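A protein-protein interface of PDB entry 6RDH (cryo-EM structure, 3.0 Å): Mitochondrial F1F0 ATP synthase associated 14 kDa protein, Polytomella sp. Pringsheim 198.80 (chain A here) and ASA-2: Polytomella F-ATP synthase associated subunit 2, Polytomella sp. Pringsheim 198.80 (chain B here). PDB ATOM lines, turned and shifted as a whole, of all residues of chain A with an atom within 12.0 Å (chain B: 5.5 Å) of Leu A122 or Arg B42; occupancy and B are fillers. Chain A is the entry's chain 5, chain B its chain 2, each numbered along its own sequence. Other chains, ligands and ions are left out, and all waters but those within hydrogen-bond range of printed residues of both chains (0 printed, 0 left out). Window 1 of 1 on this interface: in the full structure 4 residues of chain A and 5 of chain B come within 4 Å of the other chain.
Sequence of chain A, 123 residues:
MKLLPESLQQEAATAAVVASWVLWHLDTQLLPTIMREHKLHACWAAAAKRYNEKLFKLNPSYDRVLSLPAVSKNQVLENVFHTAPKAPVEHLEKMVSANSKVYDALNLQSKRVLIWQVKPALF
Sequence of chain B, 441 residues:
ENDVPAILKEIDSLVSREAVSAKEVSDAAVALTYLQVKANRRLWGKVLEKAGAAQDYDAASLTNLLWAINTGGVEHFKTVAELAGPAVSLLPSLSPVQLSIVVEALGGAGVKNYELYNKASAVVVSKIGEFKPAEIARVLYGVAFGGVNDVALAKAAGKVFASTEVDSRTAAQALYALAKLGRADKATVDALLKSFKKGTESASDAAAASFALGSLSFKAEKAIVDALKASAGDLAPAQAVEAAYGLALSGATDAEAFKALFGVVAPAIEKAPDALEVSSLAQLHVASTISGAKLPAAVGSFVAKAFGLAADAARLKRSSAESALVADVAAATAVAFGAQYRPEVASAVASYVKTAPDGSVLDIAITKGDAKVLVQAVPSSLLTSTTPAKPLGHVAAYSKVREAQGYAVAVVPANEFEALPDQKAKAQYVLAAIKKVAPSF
Of chain B, only Arg B42, Gly B45, Glu B49 and His B76 come within 4 Å of Leu A122. Arg B42 touches just these residues of chain A: Trp A116 (3.6 Å), Leu A122 (3.1 Å) and Phe A123 (3.6 Å). No residue of chain A comes within 4 Å of Asn B40. Arg B41 touches one residue of chain A. No residue of chain A comes within 4 Å of Leu B43. No residue of chain A comes within 4 Å of Lys B46. No residue of chain A comes within 4 Å of Leu B48. His B76 touches just one residue of chain A: Leu A122 (3.4 Å). Of the printed residues of chain B, Trp A116 touches Arg B42. Of the printed residues of chain B, Phe A123 touches Arg B41 (3.1 Å) and Arg B42 (3.6 Å). Printed residues of chain B within 4 Å of Ala A121: Glu B49 (3.3 Å). Pro A120 touches none of the printed residues of chain B. Val A118 touches none of the printed residues of chain B. The nearest residue of chain B that does not touch Leu A122 is Arg B41 (4.1 Å). The nearest residue of chain A that does not touch Arg B42 is Ala A121 (4.4 Å). The nearest printed residue of chain B that does not touch Phe A123 is Gly B45 (5.2 Å).
The backbone carbonyl oxygen (O) of Phe A123 lies within hydrogen-bond range of the guanidinium group (NE) of Arg B41, 3.1 Å away. The backbone carbonyl oxygen of Leu A122 lies within hydrogen-bond range of the guanidinium group of Arg B42, at 3.1 Å. The side-chain carboxylate of Glu B49 is in hydrogen-bond range of the backbone NH of Leu A122, 3.4 Å away.
OE1 of Glu B49 lies within salt-bridge range of NH1 of Arg B42, 3.5 Å away.
Of the 12 printed residues of chain A, 4 touch a printed residue of chain B. Hydrophobic or aromatic side chains of chain A within 4 Å of the printed part of chain B: Trp A116, Leu A122 and Phe A123. Hydrophobic or aromatic side chains of chain B within 4 Å of the printed part of chain A: His B76. Along chain B the printed residues that touch a printed residue of chain A span positions 41 to 76. Among the printed residues, no Asp or Glu carboxylate lies within 4 Å of a Lys or Arg side-chain nitrogen of the other chain.
Among the printed residues, pairs that only touch across the chains: Trp A116 with Arg B42 (3.6 Å), Ala A121 with Glu B49 (3.3 Å), Leu A122 with Gly B45 (3.2 Å), Leu A122 with His B76 (3.4 Å) and Phe A123 with Arg B42 (3.6 Å).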
ATOM      1  N   LEU A 108      30.411  -3.590  13.165  1.00  0.00           N
ATOM      2  CA  LEU A 108      29.837  -4.850  12.660  1.00  0.00           C
ATOM      3  C   LEU A 108      30.892  -5.881  12.289  1.00  0.00           C
ATOM      4  O   LEU A 108      30.552  -7.038  12.041  1.00  0.00           O
ATOM      5  CB  LEU A 108      28.927  -4.722  11.427  1.00  0.00           C
ATOM      6  CG  LEU A 108      27.602  -3.986  11.327  1.00  0.00           C
ATOM      7  CD1 LEU A 108      27.835  -2.726  10.565  1.00  0.00           C
ATOM      8  CD2 LEU A 108      26.569  -4.845  10.627  1.00  0.00           C
ATOM      9  N   VAL A 113      31.871  -6.022  19.282  1.00  0.00           N
ATOM     10  CA  VAL A 113      30.931  -5.031  18.771  1.00  0.00           C
ATOM     11  C   VAL A 113      29.713  -4.969  19.686  1.00  0.00           C
ATOM     12  O   VAL A 113      29.355  -5.949  20.346  1.00  0.00           O
ATOM     13  CB  VAL A 113      30.568  -5.372  17.307  1.00  0.00           C
ATOM     14  CG1 VAL A 113      29.807  -6.656  17.216  1.00  0.00           C
ATOM     15  CG2 VAL A 113      29.823  -4.252  16.619  1.00  0.00           C
ATOM     16  N   LEU A 114      29.094  -3.790  19.774  1.00  0.00           N
ATOM     17  CA  LEU A 114      27.923  -3.564  20.611  1.00  0.00           C
ATOM     18  C   LEU A 114      26.612  -3.585  19.845  1.00  0.00           C
ATOM     19  O   LEU A 114      25.656  -2.943  20.278  1.00  0.00           O
ATOM     20  CB  LEU A 114      28.027  -2.233  21.345  1.00  0.00           C
ATOM     21  CG  LEU A 114      28.643  -2.155  22.733  1.00  0.00           C
ATOM     22  CD1 LEU A 114      30.138  -2.358  22.728  1.00  0.00           C
ATOM     23  CD2 LEU A 114      28.284  -0.815  23.322  1.00  0.00           C
ATOM     24  N   ILE A 115      26.530  -4.286  18.720  1.00  0.00           N
ATOM     25  CA  ILE A 115      25.244  -4.310  18.035  1.00  0.00           C
ATOM     26  C   ILE A 115      24.351  -5.395  18.623  1.00  0.00           C
ATOM     27  O   ILE A 115      23.130  -5.238  18.680  1.00  0.00           O
ATOM     28  CB  ILE A 115      25.455  -4.454  16.517  1.00  0.00           C
ATOM     29  CG1 ILE A 115      24.133  -4.486  15.754  1.00  0.00           C
ATOM     30  CG2 ILE A 115      26.275  -5.673  16.188  1.00  0.00           C
ATOM     31  CD1 ILE A 115      23.297  -3.257  15.939  1.00  0.00           C
ATOM     32  N   TRP A 116      24.925  -6.476  19.136  1.00  0.00           N
ATOM     33  CA  TRP A 116      24.116  -7.541  19.704  1.00  0.00           C
ATOM     34  C   TRP A 116      23.779  -7.311  21.163  1.00  0.00           C
ATOM     35  O   TRP A 116      23.026  -8.098  21.737  1.00  0.00           O
ATOM     36  CB  TRP A 116      24.827  -8.877  19.521  1.00  0.00           C
ATOM     37  CG  TRP A 116      25.329  -9.024  18.135  1.00  0.00           C
ATOM     38  CD1 TRP A 116      26.618  -8.966  17.723  1.00  0.00           C
ATOM     39  CD2 TRP A 116      24.541  -9.210  16.962  1.00  0.00           C
ATOM     40  NE1 TRP A 116      26.687  -9.118  16.369  1.00  0.00           N
ATOM     41  CE2 TRP A 116      25.419  -9.266  15.877  1.00  0.00           C
ATOM     42  CE3 TRP A 116      23.172  -9.342  16.726  1.00  0.00           C
ATOM     43  CZ2 TRP A 116      24.981  -9.452  14.578  1.00  0.00           C
ATOM     44  CZ3 TRP A 116      22.738  -9.519  15.441  1.00  0.00           C
ATOM     45  CH2 TRP A 116      23.637  -9.578  14.380  1.00  0.00           C
ATOM     46  N   GLN A 117      24.304  -6.258  21.774  1.00  0.00           N
ATOM     47  CA  GLN A 117      23.907  -5.871  23.113  1.00  0.00           C
ATOM     48  C   GLN A 117      22.846  -4.796  23.097  1.00  0.00           C
ATOM     49  O   GLN A 117      22.238  -4.527  24.131  1.00  0.00           O
ATOM     50  CB  GLN A 117      25.103  -5.343  23.894  1.00  0.00           C
ATOM     51  CG  GLN A 117      26.344  -6.140  23.735  1.00  0.00           C
ATOM     52  CD  GLN A 117      27.444  -5.618  24.602  1.00  0.00           C
ATOM     53  OE1 GLN A 117      27.234  -4.714  25.400  1.00  0.00           O
ATOM     54  NE2 GLN A 117      28.638  -6.163  24.440  1.00  0.00           N
ATOM     55  N   VAL A 118      22.624  -4.185  21.951  1.00  0.00           N
ATOM     56  CA  VAL A 118      21.813  -2.990  21.824  1.00  0.00           C
ATOM     57  C   VAL A 118      20.529  -3.281  21.056  1.00  0.00           C
ATOM     58  O   VAL A 118      19.431  -3.025  21.547  1.00  0.00           O
ATOM     59  CB  VAL A 118      22.634  -1.856  21.174  1.00  0.00           C
ATOM     60  CG1 VAL A 118      21.775  -0.797  20.613  1.00  0.00           C
ATOM     61  CG2 VAL A 118      23.526  -1.246  22.212  1.00  0.00           C
ATOM     62  N   LYS A 119      20.645  -3.839  19.857  1.00  0.00           N
ATOM     63  CA  LYS A 119      19.518  -4.398  19.125  1.00  0.00           C
ATOM     64  C   LYS A 119      19.758  -5.893  19.143  1.00  0.00           C
ATOM     65  O   LYS A 119      20.477  -6.407  18.278  1.00  0.00           O
ATOM     66  CB  LYS A 119      19.454  -3.866  17.694  1.00  0.00           C
ATOM     67  CG  LYS A 119      18.910  -2.465  17.588  1.00  0.00           C
ATOM     68  CD  LYS A 119      17.496  -2.420  18.112  1.00  0.00           C
ATOM     69  CE  LYS A 119      16.837  -1.090  17.836  1.00  0.00           C
ATOM     70  NZ  LYS A 119      16.703  -0.839  16.377  1.00  0.00           N
ATOM     71  N   PRO A 120      19.179  -6.635  20.120  1.00  0.00           N
ATOM     72  CA  PRO A 120      19.777  -7.902  20.570  1.00  0.00           C
ATOM     73  C   PRO A 120      19.909  -9.011  19.540  1.00  0.00           C
ATOM     74  O   PRO A 120      21.044  -9.351  19.194  1.00  0.00           O
ATOM     75  CB  PRO A 120      18.848  -8.327  21.712  1.00  0.00           C
ATOM     76  CG  PRO A 120      17.636  -7.542  21.556  1.00  0.00           C
ATOM     77  CD  PRO A 120      18.024  -6.262  20.944  1.00  0.00           C
ATOM     78  N   ALA A 121      18.785  -9.539  19.047  1.00  0.00           N
ATOM     79  CA  ALA A 121      18.649 -10.383  17.861  1.00  0.00           C
ATOM     80  C   ALA A 121      17.179 -10.711  17.723  1.00  0.00           C
ATOM     81  O   ALA A 121      16.368 -10.271  18.538  1.00  0.00           O
ATOM     82  CB  ALA A 121      19.429 -11.695  17.922  1.00  0.00           C
ATOM     83  N   LEU A 122      16.825 -11.484  16.707  1.00  0.00           N
ATOM     84  CA  LEU A 122      15.552 -12.198  16.694  1.00  0.00           C
ATOM     85  C   LEU A 122      15.824 -13.563  16.070  1.00  0.00           C
ATOM     86  O   LEU A 122      15.851 -13.735  14.856  1.00  0.00           O
ATOM     87  CB  LEU A 122      14.457 -11.453  15.941  1.00  0.00           C
ATOM     88  CG  LEU A 122      13.546 -10.561  16.751  1.00  0.00           C
ATOM     89  CD1 LEU A 122      12.674  -9.771  15.830  1.00  0.00           C
ATOM     90  CD2 LEU A 122      12.716 -11.466  17.579  1.00  0.00           C
ATOM     91  N   PHE A 123      16.054 -14.551  16.917  1.00  0.00           N
ATOM     92  CA  PHE A 123      16.207 -15.890  16.398  1.00  0.00           C
ATOM     93  C   PHE A 123      14.948 -16.654  16.775  1.00  0.00           C
ATOM     94  O   PHE A 123      14.513 -17.543  16.053  1.00  0.00           O
ATOM     95  CB  PHE A 123      17.452 -16.584  16.948  1.00  0.00           C
ATOM     96  CG  PHE A 123      17.865 -17.798  16.156  1.00  0.00           C
ATOM     97  CD1 PHE A 123      18.748 -17.677  15.093  1.00  0.00           C
ATOM     98  CD2 PHE A 123      17.316 -19.046  16.420  1.00  0.00           C
ATOM     99  CE1 PHE A 123      19.125 -18.796  14.346  1.00  0.00           C
ATOM    100  CE2 PHE A 123      17.678 -20.160  15.677  1.00  0.00           C
ATOM    101  CZ  PHE A 123      18.579 -20.033  14.640  1.00  0.00           C
ATOM    102  N   ASN B  40      13.572 -21.823   8.602  1.00  0.00           N
ATOM    103  CA  ASN B  40      14.589 -20.807   8.862  1.00  0.00           C
ATOM    104  C   ASN B  40      13.983 -19.727   9.751  1.00  0.00           C
ATOM    105  O   ASN B  40      13.207 -18.890   9.283  1.00  0.00           O
ATOM    106  CB  ASN B  40      15.118 -20.219   7.564  1.00  0.00           C
ATOM    107  CG  ASN B  40      16.608 -20.002   7.599  1.00  0.00           C
ATOM    108  OD1 ASN B  40      17.198 -19.837   8.664  1.00  0.00           O
ATOM    109  ND2 ASN B  40      17.229 -20.010   6.431  1.00  0.00           N
ATOM    110  N   ARG B  41      14.348 -19.748  11.030  1.00  0.00           N
ATOM    111  CA  ARG B  41      13.852 -18.772  11.986  1.00  0.00           C
ATOM    112  C   ARG B  41      14.658 -17.484  11.983  1.00  0.00           C
ATOM    113  O   ARG B  41      14.108 -16.416  12.277  1.00  0.00           O
ATOM    114  CB  ARG B  41      13.868 -19.367  13.389  1.00  0.00           C
ATOM    115  CG  ARG B  41      13.179 -20.699  13.496  1.00  0.00           C
ATOM    116  CD  ARG B  41      13.469 -21.335  14.836  1.00  0.00           C
ATOM    117  NE  ARG B  41      13.282 -20.383  15.920  1.00  0.00           N
ATOM    118  CZ  ARG B  41      12.122 -20.165  16.522  1.00  0.00           C
ATOM    119  NH1 ARG B  41      12.039 -19.277  17.500  1.00  0.00           N
ATOM    120  NH2 ARG B  41      11.045 -20.833  16.142  1.00  0.00           N
ATOM    121  N   ARG B  42      15.948 -17.564  11.654  1.00  0.00           N
ATOM    122  CA  ARG B  42      16.790 -16.374  11.645  1.00  0.00           C
ATOM    123  C   ARG B  42      16.406 -15.436  10.513  1.00  0.00           C
ATOM    124  O   ARG B  42      16.483 -14.216  10.668  1.00  0.00           O
ATOM    125  CB  ARG B  42      18.258 -16.777  11.541  1.00  0.00           C
ATOM    126  CG  ARG B  42      19.260 -15.648  11.697  1.00  0.00           C
ATOM    127  CD  ARG B  42      18.931 -14.742  12.869  1.00  0.00           C
ATOM    128  NE  ARG B  42      19.842 -13.609  12.967  1.00  0.00           N
ATOM    129  CZ  ARG B  42      19.475 -12.397  13.362  1.00  0.00           C
ATOM    130  NH1 ARG B  42      18.217 -12.160  13.678  1.00  0.00           N
ATOM    131  NH2 ARG B  42      20.361 -11.419  13.428  1.00  0.00           N
ATOM    132  N   LEU B  43      15.967 -15.980   9.376  1.00  0.00           N
ATOM    133  CA  LEU B  43      15.573 -15.131   8.256  1.00  0.00           C
ATOM    134  C   LEU B  43      14.298 -14.370   8.569  1.00  0.00           C
ATOM    135  O   LEU B  43      14.176 -13.184   8.240  1.00  0.00           O
ATOM    136  CB  LEU B  43      15.383 -15.966   6.998  1.00  0.00           C
ATOM    137  CG  LEU B  43      16.509 -15.986   5.975  1.00  0.00           C
ATOM    138  CD1 LEU B  43      17.741 -16.623   6.567  1.00  0.00           C
ATOM    139  CD2 LEU B  43      16.053 -16.754   4.767  1.00  0.00           C
ATOM    140  N   TRP B  44      13.345 -15.032   9.219  1.00  0.00           N
ATOM    141  CA  TRP B  44      12.136 -14.346   9.643  1.00  0.00           C
ATOM    142  C   TRP B  44      12.431 -13.344  10.743  1.00  0.00           C
ATOM    143  O   TRP B  44      11.784 -12.295  10.812  1.00  0.00           O
ATOM    144  CB  TRP B  44      11.101 -15.355  10.106  1.00  0.00           C
ATOM    145  CG  TRP B  44      10.207 -15.792   9.023  1.00  0.00           C
ATOM    146  CD1 TRP B  44      10.185 -17.010   8.427  1.00  0.00           C
ATOM    147  CD2 TRP B  44       9.199 -15.012   8.385  1.00  0.00           C
ATOM    148  NE1 TRP B  44       9.222 -17.041   7.461  1.00  0.00           N
ATOM    149  CE2 TRP B  44       8.600 -15.824   7.417  1.00  0.00           C
ATOM    150  CE3 TRP B  44       8.740 -13.703   8.544  1.00  0.00           C
ATOM    151  CZ2 TRP B  44       7.571 -15.376   6.612  1.00  0.00           C
ATOM    152  CZ3 TRP B  44       7.717 -13.260   7.744  1.00  0.00           C
ATOM    153  CH2 TRP B  44       7.144 -14.093   6.790  1.00  0.00           C
ATOM    154  N   GLY B  45      13.429 -13.627  11.578  1.00  0.00           N
ATOM    155  CA  GLY B  45      13.852 -12.643  12.553  1.00  0.00           C
ATOM    156  C   GLY B  45      14.491 -11.420  11.927  1.00  0.00           C
ATOM    157  O   GLY B  45      14.282 -10.301  12.393  1.00  0.00           O
ATOM    158  N   LYS B  46      15.272 -11.611  10.865  1.00  0.00           N
ATOM    159  CA  LYS B  46      15.865 -10.476  10.164  1.00  0.00           C
ATOM    160  C   LYS B  46      14.800  -9.643   9.476  1.00  0.00           C
ATOM    161  O   LYS B  46      14.854  -8.405   9.503  1.00  0.00           O
ATOM    162  CB  LYS B  46      16.889 -10.953   9.142  1.00  0.00           C
ATOM    163  CG  LYS B  46      18.133 -11.572   9.722  1.00  0.00           C
ATOM    164  CD  LYS B  46      19.286 -11.402   8.769  1.00  0.00           C
ATOM    165  CE  LYS B  46      20.432 -12.328   9.090  1.00  0.00           C
ATOM    166  NZ  LYS B  46      20.213 -13.685   8.539  1.00  0.00           N
ATOM    167  N   VAL B  47      13.807 -10.305   8.879  1.00  0.00           N
ATOM    168  CA  VAL B  47      12.730  -9.588   8.208  1.00  0.00           C
ATOM    169  C   VAL B  47      11.879  -8.827   9.219  1.00  0.00           C
ATOM    170  O   VAL B  47      11.497  -7.677   8.985  1.00  0.00           O
ATOM    171  CB  VAL B  47      11.900 -10.569   7.361  1.00  0.00           C
ATOM    172  CG1 VAL B  47      10.662  -9.911   6.825  1.00  0.00           C
ATOM    173  CG2 VAL B  47      12.726 -11.073   6.220  1.00  0.00           C
ATOM    174  N   LEU B  48      11.637  -9.414  10.390  1.00  0.00           N
ATOM    175  CA  LEU B  48      10.850  -8.703  11.390  1.00  0.00           C
ATOM    176  C   LEU B  48      11.638  -7.600  12.084  1.00  0.00           C
ATOM    177  O   LEU B  48      11.051  -6.588  12.477  1.00  0.00           O
ATOM    178  CB  LEU B  48      10.284  -9.687  12.412  1.00  0.00           C
ATOM    179  CG  LEU B  48       9.017 -10.430  11.980  1.00  0.00           C
ATOM    180  CD1 LEU B  48       8.342 -11.042  13.172  1.00  0.00           C
ATOM    181  CD2 LEU B  48       8.055  -9.506  11.274  1.00  0.00           C
ATOM    182  N   GLU B  49      12.958  -7.754  12.216  1.00  0.00           N
ATOM    183  CA  GLU B  49      13.790  -6.669  12.722  1.00  0.00           C
ATOM    184  C   GLU B  49      13.782  -5.484  11.774  1.00  0.00           C
ATOM    185  O   GLU B  49      13.666  -4.332  12.207  1.00  0.00           O
ATOM    186  CB  GLU B  49      15.216  -7.156  12.920  1.00  0.00           C
ATOM    187  CG  GLU B  49      15.494  -7.733  14.269  1.00  0.00           C
ATOM    188  CD  GLU B  49      16.859  -8.362  14.336  1.00  0.00           C
ATOM    189  OE1 GLU B  49      17.357  -8.814  13.287  1.00  0.00           O
ATOM    190  OE2 GLU B  49      17.442  -8.395  15.438  1.00  0.00           O
ATOM    191  N   HIS B  76       5.654 -12.466  16.676  1.00  0.00           N
ATOM    192  CA  HIS B  76       6.495 -11.666  17.552  1.00  0.00           C
ATOM    193  C   HIS B  76       5.669 -10.446  17.902  1.00  0.00           C
ATOM    194  O   HIS B  76       5.431  -9.608  17.034  1.00  0.00           O
ATOM    195  CB  HIS B  76       7.799 -11.278  16.883  1.00  0.00           C
ATOM    196  CG  HIS B  76       8.780 -10.653  17.816  1.00  0.00           C
ATOM    197  ND1 HIS B  76       9.219  -9.357  17.674  1.00  0.00           N
ATOM    198  CD2 HIS B  76       9.387 -11.137  18.924  1.00  0.00           C
ATOM    199  CE1 HIS B  76      10.067  -9.074  18.643  1.00  0.00           C
ATOM    200  NE2 HIS B  76      10.182 -10.137  19.419  1.00  0.00           N
ATOM    201  N   THR B  79       7.108  -6.444  17.194  1.00  0.00           N
ATOM    202  CA  THR B  79       7.127  -5.815  15.877  1.00  0.00           C
ATOM    203  C   THR B  79       5.764  -5.803  15.212  1.00  0.00           C
ATOM    204  O   THR B  79       5.520  -4.958  14.349  1.00  0.00           O
ATOM    205  CB  THR B  79       8.120  -6.502  14.950  1.00  0.00           C
ATOM    206  OG1 THR B  79       7.577  -7.750  14.514  1.00  0.00           O
ATOM    207  CG2 THR B  79       9.439  -6.716  15.646  1.00  0.00           C
